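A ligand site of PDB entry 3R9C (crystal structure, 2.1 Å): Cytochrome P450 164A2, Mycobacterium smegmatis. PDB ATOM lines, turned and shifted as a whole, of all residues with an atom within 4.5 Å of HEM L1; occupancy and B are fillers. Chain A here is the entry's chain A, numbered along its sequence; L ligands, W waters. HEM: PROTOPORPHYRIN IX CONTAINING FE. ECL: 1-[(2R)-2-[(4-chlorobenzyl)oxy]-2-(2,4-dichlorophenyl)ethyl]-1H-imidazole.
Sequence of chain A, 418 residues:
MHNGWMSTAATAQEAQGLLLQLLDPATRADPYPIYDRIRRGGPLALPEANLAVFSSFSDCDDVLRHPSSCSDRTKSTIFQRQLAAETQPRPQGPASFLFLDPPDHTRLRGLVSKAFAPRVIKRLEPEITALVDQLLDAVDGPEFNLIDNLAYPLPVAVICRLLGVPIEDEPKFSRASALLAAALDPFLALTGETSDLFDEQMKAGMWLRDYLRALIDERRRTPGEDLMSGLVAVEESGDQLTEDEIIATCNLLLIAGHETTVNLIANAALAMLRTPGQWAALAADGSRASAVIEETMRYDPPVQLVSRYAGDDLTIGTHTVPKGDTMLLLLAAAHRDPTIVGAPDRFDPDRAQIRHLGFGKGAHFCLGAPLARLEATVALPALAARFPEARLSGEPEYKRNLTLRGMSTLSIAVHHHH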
ATOM      1  N   LEU A  64     -20.660   0.232   4.940  1.00  0.00           N
ATOM      2  CA  LEU A  64     -19.494  -0.385   4.330  1.00  0.00           C
ATOM      3  C   LEU A  64     -18.673  -1.221   5.314  1.00  0.00           C
ATOM      4  O   LEU A  64     -17.964  -2.138   4.902  1.00  0.00           O
ATOM      5  CB  LEU A  64     -18.610   0.673   3.652  1.00  0.00           C
ATOM      6  CG  LEU A  64     -19.195   1.378   2.415  1.00  0.00           C
ATOM      7  CD1 LEU A  64     -18.346   2.572   1.995  1.00  0.00           C
ATOM      8  CD2 LEU A  64     -19.374   0.408   1.247  1.00  0.00           C
ATOM      9  N   HIS A 105     -14.753 -14.830  -2.736  1.00  0.00           N
ATOM     10  CA  HIS A 105     -14.473 -13.424  -2.973  1.00  0.00           C
ATOM     11  C   HIS A 105     -13.056 -13.025  -2.555  1.00  0.00           C
ATOM     12  O   HIS A 105     -12.361 -12.332  -3.292  1.00  0.00           O
ATOM     13  CB  HIS A 105     -15.521 -12.573  -2.259  1.00  0.00           C
ATOM     14  CG  HIS A 105     -15.250 -11.114  -2.323  1.00  0.00           C
ATOM     15  ND1 HIS A 105     -14.786 -10.400  -1.234  1.00  0.00           N
ATOM     16  CD2 HIS A 105     -15.340 -10.231  -3.345  1.00  0.00           C
ATOM     17  CE1 HIS A 105     -14.615  -9.141  -1.584  1.00  0.00           C
ATOM     18  NE2 HIS A 105     -14.957  -9.003  -2.856  1.00  0.00           N
ATOM     19  N   ARG A 109     -10.015 -11.736  -5.058  1.00  0.00           N
ATOM     20  CA  ARG A 109      -9.313 -10.482  -4.757  1.00  0.00           C
ATOM     21  C   ARG A 109      -7.811 -10.687  -4.621  1.00  0.00           C
ATOM     22  O   ARG A 109      -7.035  -9.887  -5.128  1.00  0.00           O
ATOM     23  CB  ARG A 109      -9.859  -9.848  -3.483  1.00  0.00           C
ATOM     24  CG  ARG A 109     -10.974  -8.868  -3.721  1.00  0.00           C
ATOM     25  CD  ARG A 109     -11.404  -8.233  -2.408  1.00  0.00           C
ATOM     26  NE  ARG A 109     -10.481  -7.215  -1.920  1.00  0.00           N
ATOM     27  CZ  ARG A 109     -10.454  -5.949  -2.333  1.00  0.00           C
ATOM     28  NH1 ARG A 109     -11.288  -5.525  -3.274  1.00  0.00           N
ATOM     29  NH2 ARG A 109      -9.583  -5.099  -1.804  1.00  0.00           N
ATOM     30  N   PHE A 116      -2.603  -5.975  -9.801  1.00  0.00           N
ATOM     31  CA  PHE A 116      -2.964  -4.558  -9.708  1.00  0.00           C
ATOM     32  C   PHE A 116      -2.261  -3.788  -8.591  1.00  0.00           C
ATOM     33  O   PHE A 116      -2.577  -2.617  -8.338  1.00  0.00           O
ATOM     34  CB  PHE A 116      -4.485  -4.393  -9.631  1.00  0.00           C
ATOM     35  CG  PHE A 116      -5.162  -4.521 -10.964  1.00  0.00           C
ATOM     36  CD1 PHE A 116      -5.397  -3.397 -11.749  1.00  0.00           C
ATOM     37  CD2 PHE A 116      -5.563  -5.776 -11.441  1.00  0.00           C
ATOM     38  CE1 PHE A 116      -6.016  -3.517 -12.996  1.00  0.00           C
ATOM     39  CE2 PHE A 116      -6.179  -5.892 -12.674  1.00  0.00           C
ATOM     40  CZ  PHE A 116      -6.411  -4.760 -13.454  1.00  0.00           C
ATOM     41  N   ILE A 159      -6.522  -0.820 -20.812  1.00  0.00           N
ATOM     42  CA  ILE A 159      -7.264  -2.035 -20.450  1.00  0.00           C
ATOM     43  C   ILE A 159      -7.271  -3.093 -21.566  1.00  0.00           C
ATOM     44  O   ILE A 159      -7.197  -4.294 -21.274  1.00  0.00           O
ATOM     45  CB  ILE A 159      -8.711  -1.737 -19.928  1.00  0.00           C
ATOM     46  CG1 ILE A 159      -9.239  -2.887 -19.070  1.00  0.00           C
ATOM     47  CG2 ILE A 159      -9.680  -1.416 -21.068  1.00  0.00           C
ATOM     48  CD1 ILE A 159      -8.532  -3.040 -17.731  1.00  0.00           C
ATOM     49  N   LEU A 252     -15.828  -7.342 -15.145  1.00  0.00           N
ATOM     50  CA  LEU A 252     -15.633  -6.255 -14.201  1.00  0.00           C
ATOM     51  C   LEU A 252     -14.520  -5.318 -14.670  1.00  0.00           C
ATOM     52  O   LEU A 252     -14.721  -4.102 -14.729  1.00  0.00           O
ATOM     53  CB  LEU A 252     -15.340  -6.801 -12.800  1.00  0.00           C
ATOM     54  CG  LEU A 252     -15.414  -5.803 -11.637  1.00  0.00           C
ATOM     55  CD1 LEU A 252     -15.671  -6.514 -10.316  1.00  0.00           C
ATOM     56  CD2 LEU A 252     -14.157  -4.960 -11.558  1.00  0.00           C
ATOM     57  N   LEU A 253     -13.371  -5.901 -14.994  1.00  0.00           N
ATOM     58  CA  LEU A 253     -12.187  -5.126 -15.393  1.00  0.00           C
ATOM     59  C   LEU A 253     -12.382  -4.341 -16.692  1.00  0.00           C
ATOM     60  O   LEU A 253     -11.912  -3.208 -16.807  1.00  0.00           O
ATOM     61  CB  LEU A 253     -10.963  -6.039 -15.524  1.00  0.00           C
ATOM     62  CG  LEU A 253     -10.441  -6.777 -14.290  1.00  0.00           C
ATOM     63  CD1 LEU A 253      -9.229  -7.622 -14.669  1.00  0.00           C
ATOM     64  CD2 LEU A 253     -10.089  -5.822 -13.134  1.00  0.00           C
ATOM     65  N   ALA A 256     -14.692  -1.436 -15.953  1.00  0.00           N
ATOM     66  CA  ALA A 256     -13.881  -0.497 -15.177  1.00  0.00           C
ATOM     67  C   ALA A 256     -12.925   0.273 -16.088  1.00  0.00           C
ATOM     68  O   ALA A 256     -12.734   1.482 -15.924  1.00  0.00           O
ATOM     69  CB  ALA A 256     -13.103  -1.241 -14.096  1.00  0.00           C
ATOM     70  N   GLY A 257     -12.354  -0.433 -17.072  1.00  0.00           N
ATOM     71  CA  GLY A 257     -11.419   0.170 -18.012  1.00  0.00           C
ATOM     72  C   GLY A 257     -12.034   1.167 -18.977  1.00  0.00           C
ATOM     73  O   GLY A 257     -11.355   2.053 -19.498  1.00  0.00           O
ATOM     74  N   THR A 260     -14.742   4.420 -16.014  1.00  0.00           N
ATOM     75  CA  THR A 260     -14.379   4.962 -14.700  1.00  0.00           C
ATOM     76  C   THR A 260     -13.327   6.067 -14.759  1.00  0.00           C
ATOM     77  O   THR A 260     -13.645   7.223 -14.478  1.00  0.00           O
ATOM     78  CB  THR A 260     -13.939   3.864 -13.688  1.00  0.00           C
ATOM     79  OG1 THR A 260     -12.759   3.209 -14.179  1.00  0.00           O
ATOM     80  CG2 THR A 260     -15.045   2.850 -13.468  1.00  0.00           C
ATOM     81  N   THR A 261     -12.089   5.716 -15.106  1.00  0.00           N
ATOM     82  CA  THR A 261     -11.004   6.702 -15.153  1.00  0.00           C
ATOM     83  C   THR A 261     -11.332   7.869 -16.079  1.00  0.00           C
ATOM     84  O   THR A 261     -10.950   9.007 -15.796  1.00  0.00           O
ATOM     85  CB  THR A 261      -9.655   6.080 -15.574  1.00  0.00           C
ATOM     86  OG1 THR A 261      -9.433   4.860 -14.861  1.00  0.00           O
ATOM     87  CG2 THR A 261      -8.507   7.047 -15.272  1.00  0.00           C
ATOM     88  N   LEU A 264     -12.833  10.383 -13.929  1.00  0.00           N
ATOM     89  CA  LEU A 264     -11.874  11.009 -13.031  1.00  0.00           C
ATOM     90  C   LEU A 264     -11.091  12.098 -13.770  1.00  0.00           C
ATOM     91  O   LEU A 264     -10.947  13.213 -13.272  1.00  0.00           O
ATOM     92  CB  LEU A 264     -10.925   9.975 -12.410  1.00  0.00           C
ATOM     93  CG  LEU A 264      -9.730  10.509 -11.592  1.00  0.00           C
ATOM     94  CD1 LEU A 264     -10.174  11.419 -10.439  1.00  0.00           C
ATOM     95  CD2 LEU A 264      -8.877   9.352 -11.072  1.00  0.00           C
ATOM     96  N   MET A 297     -11.981  13.233  -6.614  1.00  0.00           N
ATOM     97  CA  MET A 297     -12.600  12.031  -6.057  1.00  0.00           C
ATOM     98  C   MET A 297     -13.627  12.377  -4.977  1.00  0.00           C
ATOM     99  O   MET A 297     -14.682  11.745  -4.880  1.00  0.00           O
ATOM    100  CB  MET A 297     -11.546  11.075  -5.503  1.00  0.00           C
ATOM    101  CG  MET A 297     -10.687  10.389  -6.571  1.00  0.00           C
ATOM    102  SD  MET A 297     -11.617   9.328  -7.700  1.00  0.00           S
ATOM    103  CE  MET A 297     -12.325   8.163  -6.540  1.00  0.00           C
ATOM    104  N   PRO A 302     -16.408   9.908  -9.706  1.00  0.00           N
ATOM    105  CA  PRO A 302     -16.757   9.113 -10.894  1.00  0.00           C
ATOM    106  C   PRO A 302     -17.820   8.046 -10.599  1.00  0.00           C
ATOM    107  O   PRO A 302     -18.711   7.824 -11.426  1.00  0.00           O
ATOM    108  CB  PRO A 302     -15.430   8.461 -11.279  1.00  0.00           C
ATOM    109  CG  PRO A 302     -14.398   9.402 -10.776  1.00  0.00           C
ATOM    110  CD  PRO A 302     -14.947   9.912  -9.471  1.00  0.00           C
ATOM    111  N   VAL A 303     -17.698   7.384  -9.443  1.00  0.00           N
ATOM    112  CA  VAL A 303     -18.721   6.465  -8.953  1.00  0.00           C
ATOM    113  C   VAL A 303     -19.514   7.193  -7.877  1.00  0.00           C
ATOM    114  O   VAL A 303     -18.969   7.520  -6.817  1.00  0.00           O
ATOM    115  CB  VAL A 303     -18.114   5.147  -8.379  1.00  0.00           C
ATOM    116  CG1 VAL A 303     -19.207   4.227  -7.844  1.00  0.00           C
ATOM    117  CG2 VAL A 303     -17.282   4.433  -9.432  1.00  0.00           C
ATOM    118  N   VAL A 306     -22.911   3.381  -4.205  1.00  0.00           N
ATOM    119  CA  VAL A 306     -22.788   1.934  -4.150  1.00  0.00           C
ATOM    120  C   VAL A 306     -23.995   1.356  -3.421  1.00  0.00           C
ATOM    121  O   VAL A 306     -24.772   2.097  -2.808  1.00  0.00           O
ATOM    122  CB  VAL A 306     -21.472   1.462  -3.444  1.00  0.00           C
ATOM    123  CG1 VAL A 306     -20.261   1.803  -4.292  1.00  0.00           C
ATOM    124  CG2 VAL A 306     -21.360   2.063  -2.030  1.00  0.00           C
ATOM    125  N   ARG A 308     -25.456  -2.126  -0.892  1.00  0.00           N
ATOM    126  CA  ARG A 308     -25.241  -3.322  -0.099  1.00  0.00           C
ATOM    127  C   ARG A 308     -26.611  -3.875   0.265  1.00  0.00           C
ATOM    128  O   ARG A 308     -27.614  -3.161   0.202  1.00  0.00           O
ATOM    129  CB  ARG A 308     -24.451  -3.010   1.186  1.00  0.00           C
ATOM    130  CG  ARG A 308     -22.980  -2.610   0.988  1.00  0.00           C
ATOM    131  CD  ARG A 308     -22.122  -3.785   0.524  1.00  0.00           C
ATOM    132  NE  ARG A 308     -20.703  -3.435   0.468  1.00  0.00           N
ATOM    133  CZ  ARG A 308     -20.099  -2.857  -0.563  1.00  0.00           C
ATOM    134  NH1 ARG A 308     -20.792  -2.547  -1.656  1.00  0.00           N
ATOM    135  NH2 ARG A 308     -18.802  -2.589  -0.501  1.00  0.00           N
ATOM    136  N   LEU A 357     -14.507   8.202   0.259  1.00  0.00           N
ATOM    137  CA  LEU A 357     -15.011   6.865  -0.006  1.00  0.00           C
ATOM    138  C   LEU A 357     -15.123   6.559  -1.499  1.00  0.00           C
ATOM    139  O   LEU A 357     -15.808   5.604  -1.893  1.00  0.00           O
ATOM    140  CB  LEU A 357     -16.372   6.670   0.686  1.00  0.00           C
ATOM    141  CG  LEU A 357     -16.420   6.800   2.210  1.00  0.00           C
ATOM    142  CD1 LEU A 357     -17.860   6.894   2.696  1.00  0.00           C
ATOM    143  CD2 LEU A 357     -15.680   5.655   2.906  1.00  0.00           C
ATOM    144  N   GLY A 358     -14.440   7.358  -2.312  1.00  0.00           N
ATOM    145  CA  GLY A 358     -14.548   7.277  -3.770  1.00  0.00           C
ATOM    146  C   GLY A 358     -14.054   5.987  -4.398  1.00  0.00           C
ATOM    147  O   GLY A 358     -14.470   5.633  -5.513  1.00  0.00           O
ATOM    148  N   PHE A 359     -13.162   5.294  -3.699  1.00  0.00           N
ATOM    149  CA  PHE A 359     -12.685   3.980  -4.141  1.00  0.00           C
ATOM    150  C   PHE A 359     -13.265   2.878  -3.248  1.00  0.00           C
ATOM    151  O   PHE A 359     -12.778   1.750  -3.253  1.00  0.00           O
ATOM    152  CB  PHE A 359     -11.156   3.922  -4.162  1.00  0.00           C
ATOM    153  CG  PHE A 359     -10.519   4.726  -5.265  1.00  0.00           C
ATOM    154  CD1 PHE A 359     -10.729   4.391  -6.600  1.00  0.00           C
ATOM    155  CD2 PHE A 359      -9.694   5.804  -4.967  1.00  0.00           C
ATOM    156  CE1 PHE A 359     -10.141   5.131  -7.620  1.00  0.00           C
ATOM    157  CE2 PHE A 359      -9.092   6.547  -5.977  1.00  0.00           C
ATOM    158  CZ  PHE A 359      -9.321   6.213  -7.306  1.00  0.00           C
ATOM    159  N   GLY A 360     -14.306   3.231  -2.491  1.00  0.00           N
ATOM    160  CA  GLY A 360     -14.925   2.309  -1.532  1.00  0.00           C
ATOM    161  C   GLY A 360     -14.029   2.151  -0.326  1.00  0.00           C
ATOM    162  O   GLY A 360     -13.182   3.016  -0.050  1.00  0.00           O
ATOM    163  N   ALA A 363     -13.430  -4.658   2.553  1.00  0.00           N
ATOM    164  CA  ALA A 363     -13.299  -5.895   1.796  1.00  0.00           C
ATOM    165  C   ALA A 363     -13.521  -5.730   0.298  1.00  0.00           C
ATOM    166  O   ALA A 363     -13.101  -6.581  -0.489  1.00  0.00           O
ATOM    167  CB  ALA A 363     -14.225  -6.965   2.369  1.00  0.00           C
ATOM    168  N   HIS A 364     -14.151  -4.629  -0.102  1.00  0.00           N
ATOM    169  CA  HIS A 364     -14.470  -4.391  -1.512  1.00  0.00           C
ATOM    170  C   HIS A 364     -13.734  -3.197  -2.133  1.00  0.00           C
ATOM    171  O   HIS A 364     -14.097  -2.735  -3.212  1.00  0.00           O
ATOM    172  CB  HIS A 364     -15.984  -4.231  -1.687  1.00  0.00           C
ATOM    173  CG  HIS A 364     -16.786  -5.344  -1.081  1.00  0.00           C
ATOM    174  ND1 HIS A 364     -17.008  -6.533  -1.727  1.00  0.00           N
ATOM    175  CD2 HIS A 364     -17.404  -5.448   0.128  1.00  0.00           C
ATOM    176  CE1 HIS A 364     -17.723  -7.327  -0.951  1.00  0.00           C
ATOM    177  NE2 HIS A 364     -17.983  -6.691   0.166  1.00  0.00           N
ATOM    178  N   PHE A 365     -12.695  -2.709  -1.446  1.00  0.00           N
ATOM    179  CA  PHE A 365     -11.932  -1.544  -1.909  1.00  0.00           C
ATOM    180  C   PHE A 365     -11.437  -1.722  -3.338  1.00  0.00           C
ATOM    181  O   PHE A 365     -11.026  -2.818  -3.729  1.00  0.00           O
ATOM    182  CB  PHE A 365     -10.755  -1.231  -0.971  1.00  0.00           C
ATOM    183  CG  PHE A 365     -10.040   0.067  -1.284  1.00  0.00           C
ATOM    184  CD1 PHE A 365     -10.502   1.278  -0.791  1.00  0.00           C
ATOM    185  CD2 PHE A 365      -8.878   0.063  -2.072  1.00  0.00           C
ATOM    186  CE1 PHE A 365      -9.843   2.476  -1.079  1.00  0.00           C
ATOM    187  CE2 PHE A 365      -8.207   1.257  -2.354  1.00  0.00           C
ATOM    188  CZ  PHE A 365      -8.691   2.473  -1.863  1.00  0.00           C
ATOM    189  N   CYS A 366     -11.484  -0.646  -4.123  1.00  0.00           N
ATOM    190  CA  CYS A 366     -11.109  -0.668  -5.539  1.00  0.00           C
ATOM    191  C   CYS A 366      -9.671  -1.121  -5.778  1.00  0.00           C
ATOM    192  O   CYS A 366      -8.720  -0.437  -5.392  1.00  0.00           O
ATOM    193  CB  CYS A 366     -11.319   0.699  -6.185  1.00  0.00           C
ATOM    194  SG  CYS A 366     -10.969   0.696  -7.962  1.00  0.00           S
ATOM    195  N   LEU A 367      -9.517  -2.275  -6.426  1.00  0.00           N
ATOM    196  CA  LEU A 367      -8.186  -2.772  -6.773  1.00  0.00           C
ATOM    197  C   LEU A 367      -7.566  -2.004  -7.931  1.00  0.00           C
ATOM    198  O   LEU A 367      -6.354  -2.056  -8.138  1.00  0.00           O
ATOM    199  CB  LEU A 367      -8.233  -4.272  -7.071  1.00  0.00           C
ATOM    200  CG  LEU A 367      -8.576  -5.201  -5.891  1.00  0.00           C
ATOM    201  CD1 LEU A 367      -8.479  -6.661  -6.303  1.00  0.00           C
ATOM    202  CD2 LEU A 367      -7.684  -4.923  -4.683  1.00  0.00           C
ATOM    203  N   GLY A 368      -8.394  -1.286  -8.694  1.00  0.00           N
ATOM    204  CA  GLY A 368      -7.906  -0.485  -9.805  1.00  0.00           C
ATOM    205  C   GLY A 368      -7.490   0.916  -9.422  1.00  0.00           C
ATOM    206  O   GLY A 368      -7.063   1.689 -10.286  1.00  0.00           O
ATOM    207  N   LEU A 371      -4.037   2.064 -10.627  1.00  0.00           N
ATOM    208  CA  LEU A 371      -4.044   2.275 -12.073  1.00  0.00           C
ATOM    209  C   LEU A 371      -4.773   3.554 -12.464  1.00  0.00           C
ATOM    210  O   LEU A 371      -4.266   4.337 -13.272  1.00  0.00           O
ATOM    211  CB  LEU A 371      -4.612   1.064 -12.828  1.00  0.00           C
ATOM    212  CG  LEU A 371      -4.738   1.178 -14.351  1.00  0.00           C
ATOM    213  CD1 LEU A 371      -3.395   1.433 -15.036  1.00  0.00           C
ATOM    214  CD2 LEU A 371      -5.407  -0.076 -14.920  1.00  0.00           C
ATOM    215  N   ALA A 372      -5.957   3.762 -11.894  1.00  0.00           N
ATOM    216  CA  ALA A 372      -6.759   4.960 -12.144  1.00  0.00           C
ATOM    217  C   ALA A 372      -5.996   6.238 -11.783  1.00  0.00           C
ATOM    218  O   ALA A 372      -5.954   7.186 -12.580  1.00  0.00           O
ATOM    219  CB  ALA A 372      -8.069   4.889 -11.361  1.00  0.00           C
HETATM  220  CHA HEM L   1     -14.376  -1.706  -6.761  1.00  0.00           C
HETATM  221  CHB HEM L   1     -14.446   3.026  -7.842  1.00  0.00           C
HETATM  222  CHC HEM L   1     -11.383   2.221 -11.529  1.00  0.00           C
HETATM  223  CHD HEM L   1     -11.157  -2.488 -10.381  1.00  0.00           C
HETATM  224  C1A HEM L   1     -14.664  -0.358  -6.697  1.00  0.00           C
HETATM  225  C2A HEM L   1     -15.473   0.329  -5.705  1.00  0.00           C
HETATM  226  C3A HEM L   1     -15.486   1.632  -6.009  1.00  0.00           C
HETATM  227  C4A HEM L   1     -14.685   1.821  -7.203  1.00  0.00           C
HETATM  228  CMA HEM L   1     -16.220   2.752  -5.236  1.00  0.00           C
HETATM  229  CAA HEM L   1     -16.193  -0.340  -4.502  1.00  0.00           C
HETATM  230  CBA HEM L   1     -17.491  -1.003  -4.931  1.00  0.00           C
HETATM  231  CGA HEM L   1     -18.356  -1.333  -3.736  1.00  0.00           C
HETATM  232  O1A HEM L   1     -17.940  -1.122  -2.578  1.00  0.00           O
HETATM  233  O2A HEM L   1     -19.501  -1.828  -3.941  1.00  0.00           O
HETATM  234  C1B HEM L   1     -13.595   3.247  -8.907  1.00  0.00           C
HETATM  235  C2B HEM L   1     -13.229   4.526  -9.474  1.00  0.00           C
HETATM  236  C3B HEM L   1     -12.380   4.308 -10.493  1.00  0.00           C
HETATM  237  C4B HEM L   1     -12.180   2.872 -10.600  1.00  0.00           C
HETATM  238  CMB HEM L   1     -13.751   5.901  -8.979  1.00  0.00           C
HETATM  239  CAB HEM L   1     -11.718   5.355 -11.420  1.00  0.00           C
HETATM  240  CBB HEM L   1     -11.218   6.504 -10.956  1.00  0.00           C
HETATM  241  C1C HEM L   1     -11.064   0.881 -11.560  1.00  0.00           C
HETATM  242  C2C HEM L   1     -10.218   0.223 -12.533  1.00  0.00           C
HETATM  243  C3C HEM L   1     -10.160  -1.082 -12.219  1.00  0.00           C
HETATM  244  C4C HEM L   1     -10.965  -1.297 -11.040  1.00  0.00           C
HETATM  245  CMC HEM L   1      -9.526   0.929 -13.728  1.00  0.00           C
HETATM  246  CAC HEM L   1      -9.385  -2.194 -12.961  1.00  0.00           C
HETATM  247  CBC HEM L   1      -9.606  -2.427 -14.264  1.00  0.00           C
HETATM  248  C1D HEM L   1     -12.027  -2.746  -9.346  1.00  0.00           C
HETATM  249  C2D HEM L   1     -12.348  -4.049  -8.833  1.00  0.00           C
HETATM  250  C3D HEM L   1     -13.352  -3.793  -7.708  1.00  0.00           C
HETATM  251  C4D HEM L   1     -13.545  -2.367  -7.645  1.00  0.00           C
HETATM  252  CMD HEM L   1     -11.789  -5.418  -9.311  1.00  0.00           C
HETATM  253  CAD HEM L   1     -14.045  -4.865  -6.848  1.00  0.00           C
HETATM  254  CBD HEM L   1     -13.276  -5.145  -5.574  1.00  0.00           C
HETATM  255  CGD HEM L   1     -14.125  -6.110  -4.784  1.00  0.00           C
HETATM  256  O1D HEM L   1     -13.598  -6.733  -3.845  1.00  0.00           O
HETATM  257  O2D HEM L   1     -15.343  -6.272  -5.071  1.00  0.00           O
HETATM  258  NA  HEM L   1     -14.209   0.586  -7.581  1.00  0.00           N
HETATM  259  NB  HEM L   1     -12.934   2.268  -9.616  1.00  0.00           N
HETATM  260  NC  HEM L   1     -11.497  -0.082 -10.671  1.00  0.00           N
HETATM  261  ND  HEM L   1     -12.748  -1.796  -8.627  1.00  0.00           N
HETATM  262 FE   HEM L   1     -12.862   0.227  -9.121  1.00  0.00          FE
HETATM  263  C1  ECL L   2     -19.886  -5.426 -12.789  1.00  0.00           C
HETATM  264  N1  ECL L   2     -16.086  -0.977 -11.607  1.00  0.00           N
HETATM  265  C2  ECL L   2     -19.765  -5.067 -14.127  1.00  0.00           C
HETATM  266 CL2  ECL L   2     -22.331  -7.572 -16.007  1.00  0.00          CL
HETATM  267  C3  ECL L   2     -14.932  -1.246 -10.992  1.00  0.00           C
HETATM  268 CL4  ECL L   2     -20.929   1.133  -7.812  1.00  0.00          CL
HETATM  269  C5  ECL L   2     -20.430  -0.179 -10.213  1.00  0.00           C
HETATM  270  C6  ECL L   2     -15.403   0.848 -10.634  1.00  0.00           C
HETATM  271  C7  ECL L   2     -16.403   0.302 -11.395  1.00  0.00           C
HETATM  272  C8  ECL L   2     -19.073  -4.698 -11.757  1.00  0.00           C
HETATM  273 CL8  ECL L   2     -16.808  -2.390  -8.516  1.00  0.00          CL
HETATM  274  C9  ECL L   2     -21.520  -7.103 -13.385  1.00  0.00           C
HETATM  275  C10 ECL L   2     -20.777  -6.435 -12.408  1.00  0.00           C
HETATM  276  C11 ECL L   2     -21.389  -6.745 -14.727  1.00  0.00           C
HETATM  277  C13 ECL L   2     -20.516  -5.727 -15.096  1.00  0.00           C
HETATM  278  C14 ECL L   2     -20.037   0.010  -8.891  1.00  0.00           C
HETATM  279  C15 ECL L   2     -18.923  -0.665  -8.393  1.00  0.00           C
HETATM  280  C16 ECL L   2     -18.219  -1.542  -9.208  1.00  0.00           C
HETATM  281  C17 ECL L   2     -18.604  -1.740 -10.537  1.00  0.00           C
HETATM  282  C19 ECL L   2     -16.891  -1.932 -12.359  1.00  0.00           C
HETATM  283  N19 ECL L   2     -14.506  -0.129 -10.391  1.00  0.00           N
HETATM  284  C20 ECL L   2     -17.861  -2.676 -11.426  1.00  0.00           C
HETATM  285  O20 ECL L   2     -18.777  -3.391 -12.248  1.00  0.00           O
HETATM  286  C21 ECL L   2     -19.715  -1.048 -11.025  1.00  0.00           C
HETATM  287  C1  ECL L   3     -15.370 -10.249  -8.410  1.00  0.00           C
HETATM  288  N1  ECL L   3     -19.757  -8.969  -6.800  1.00  0.00           N
HETATM  289  C2  ECL L   3     -14.352 -10.663  -9.274  1.00  0.00           C
HETATM  290 CL2  ECL L   3     -11.071  -8.904  -7.660  1.00  0.00          CL
HETATM  291  C3  ECL L   3     -19.025  -8.126  -6.075  1.00  0.00           C
HETATM  292 CL4  ECL L   3     -20.214 -10.477 -14.797  1.00  0.00          CL
HETATM  293  C5  ECL L   3     -18.875  -9.428 -12.630  1.00  0.00           C
HETATM  294  C6  ECL L   3     -19.882  -9.600  -4.704  1.00  0.00           C
HETATM  295  C7  ECL L   3     -20.295  -9.890  -5.987  1.00  0.00           C
HETATM  296  C8  ECL L   3     -16.786 -10.694  -8.650  1.00  0.00           C
HETATM  297 CL8  ECL L   3     -21.214 -11.921  -9.556  1.00  0.00          CL
HETATM  298  C9  ECL L   3     -13.763  -9.020  -7.089  1.00  0.00           C
HETATM  299  C10 ECL L   3     -15.069  -9.426  -7.312  1.00  0.00           C
HETATM  300  C11 ECL L   3     -12.757  -9.428  -7.959  1.00  0.00           C
HETATM  301  C13 ECL L   3     -13.044 -10.248  -9.046  1.00  0.00           C
HETATM  302  C14 ECL L   3     -19.859 -10.310 -13.048  1.00  0.00           C
HETATM  303  C15 ECL L   3     -20.568 -11.069 -12.116  1.00  0.00           C
HETATM  304  C16 ECL L   3     -20.291 -10.950 -10.757  1.00  0.00           C
HETATM  305  C17 ECL L   3     -19.307 -10.054 -10.341  1.00  0.00           C
HETATM  306  C19 ECL L   3     -19.923  -8.891  -8.249  1.00  0.00           C
HETATM  307  N19 ECL L   3     -19.096  -8.505  -4.777  1.00  0.00           N
HETATM  308  C20 ECL L   3     -19.003  -9.922  -8.895  1.00  0.00           C
HETATM  309  O20 ECL L   3     -17.640  -9.552  -8.688  1.00  0.00           O
HETATM  310  C21 ECL L   3     -18.598  -9.295 -11.274  1.00  0.00           C
HETATM  311  O   HOH W   1     -15.921  -0.934  -0.889  1.00  0.00           O
HETATM  312  O   HOH W   2     -10.253   2.865 -16.518  1.00  0.00           O
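A nitrogen (N19) of ECL L2 binds an iron atom (FE) of HEM L1 (2.1 Å).
The backbone carbonyl oxygen (O) of Ala 363 sits close to an oxygen (O1D) of HEM L1, 3.4 Å away.
Merely in contact with HEM L1: Phe 116 (3.6 Å), Ile 159 (3.7 Å), Leu 252 (3.3 Å), Leu 253 (3.5 Å), Ala 256 (3.5 Å), Thr 260 (3.1 Å), Thr 261 (3.7 Å), Leu 264 (3.7 Å), Met 297 (3.6 Å), Pro 302 (3.8 Å), Val 303 (3.5 Å), Val 306 (3.7 Å), Gly 358 (3.4 Å), Phe 359 (3.6 Å), Gly 360 (3.4 Å), His 364 (3.4 Å), Phe 365 (3.7 Å), Leu 367 (3.9 Å), Gly 368 (3.4 Å) and Ala 372 (3.6 Å).
Within 4 Å of HEM L1: His 105, Arg 109, Phe 116, Ile 159, Leu 252, Leu 253, Ala 256, Thr 260, Thr 261, Leu 264, Met 297, Pro 302, Val 303, Val 306, Arg 308, Gly 358, Phe 359, Gly 360, Ala 363, His 364, Phe 365, Cys 366, Leu 367, Gly 368 and Ala 372.
The nearest printed residue that does not touch HEM L1 is Leu 64 (4.4 Å).
FE of HEM L1 is bound by SG of Cys 366, at 2.3 Å.
An oxygen (O1D) of HEM L1 is in salt-bridge range of the guanidinium group (NH1) of Arg 109 (2.7 Å).
The guanidinium group (NH2) of Arg 308 lies within salt-bridge range of an oxygen (O1A) of HEM L1 (2.7 Å).
O1D of HEM L1 sits at hydrogen-bond distance from NE2 of His 105 (2.8 Å).
The side-chain sulfur (SG) of Cys 366 sits close to the backbone NH (N) of Gly 368, 3.3 Å away.
The backbone NH (N) of Cys 366 lies within hydrogen-bond range of the backbone carbonyl oxygen (O) of Phe 359, at 2.9 Å.
NE of Arg 109 sits close to O of Ala 363.
NH1 of Arg 109 sits at hydrogen-bond distance from O of Phe 365 (2.8 Å).
NE2 of His 105 lies within hydrogen-bond range of ND1 of His 364, 3.4 Å away.
The side-chain hydroxyl (OG1) of Thr 260 sits at hydrogen-bond distance from the backbone carbonyl oxygen (O) of Ala 256, at 2.5 Å.
Water W1 lies within hydrogen-bond range of O1A of HEM L1, NH2 of Arg 308 and O of His 364.
Water W2 lies within hydrogen-bond range of OG1 of Thr 261, O of Ala 256, O of Gly 257 and OG1 of Thr 260.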
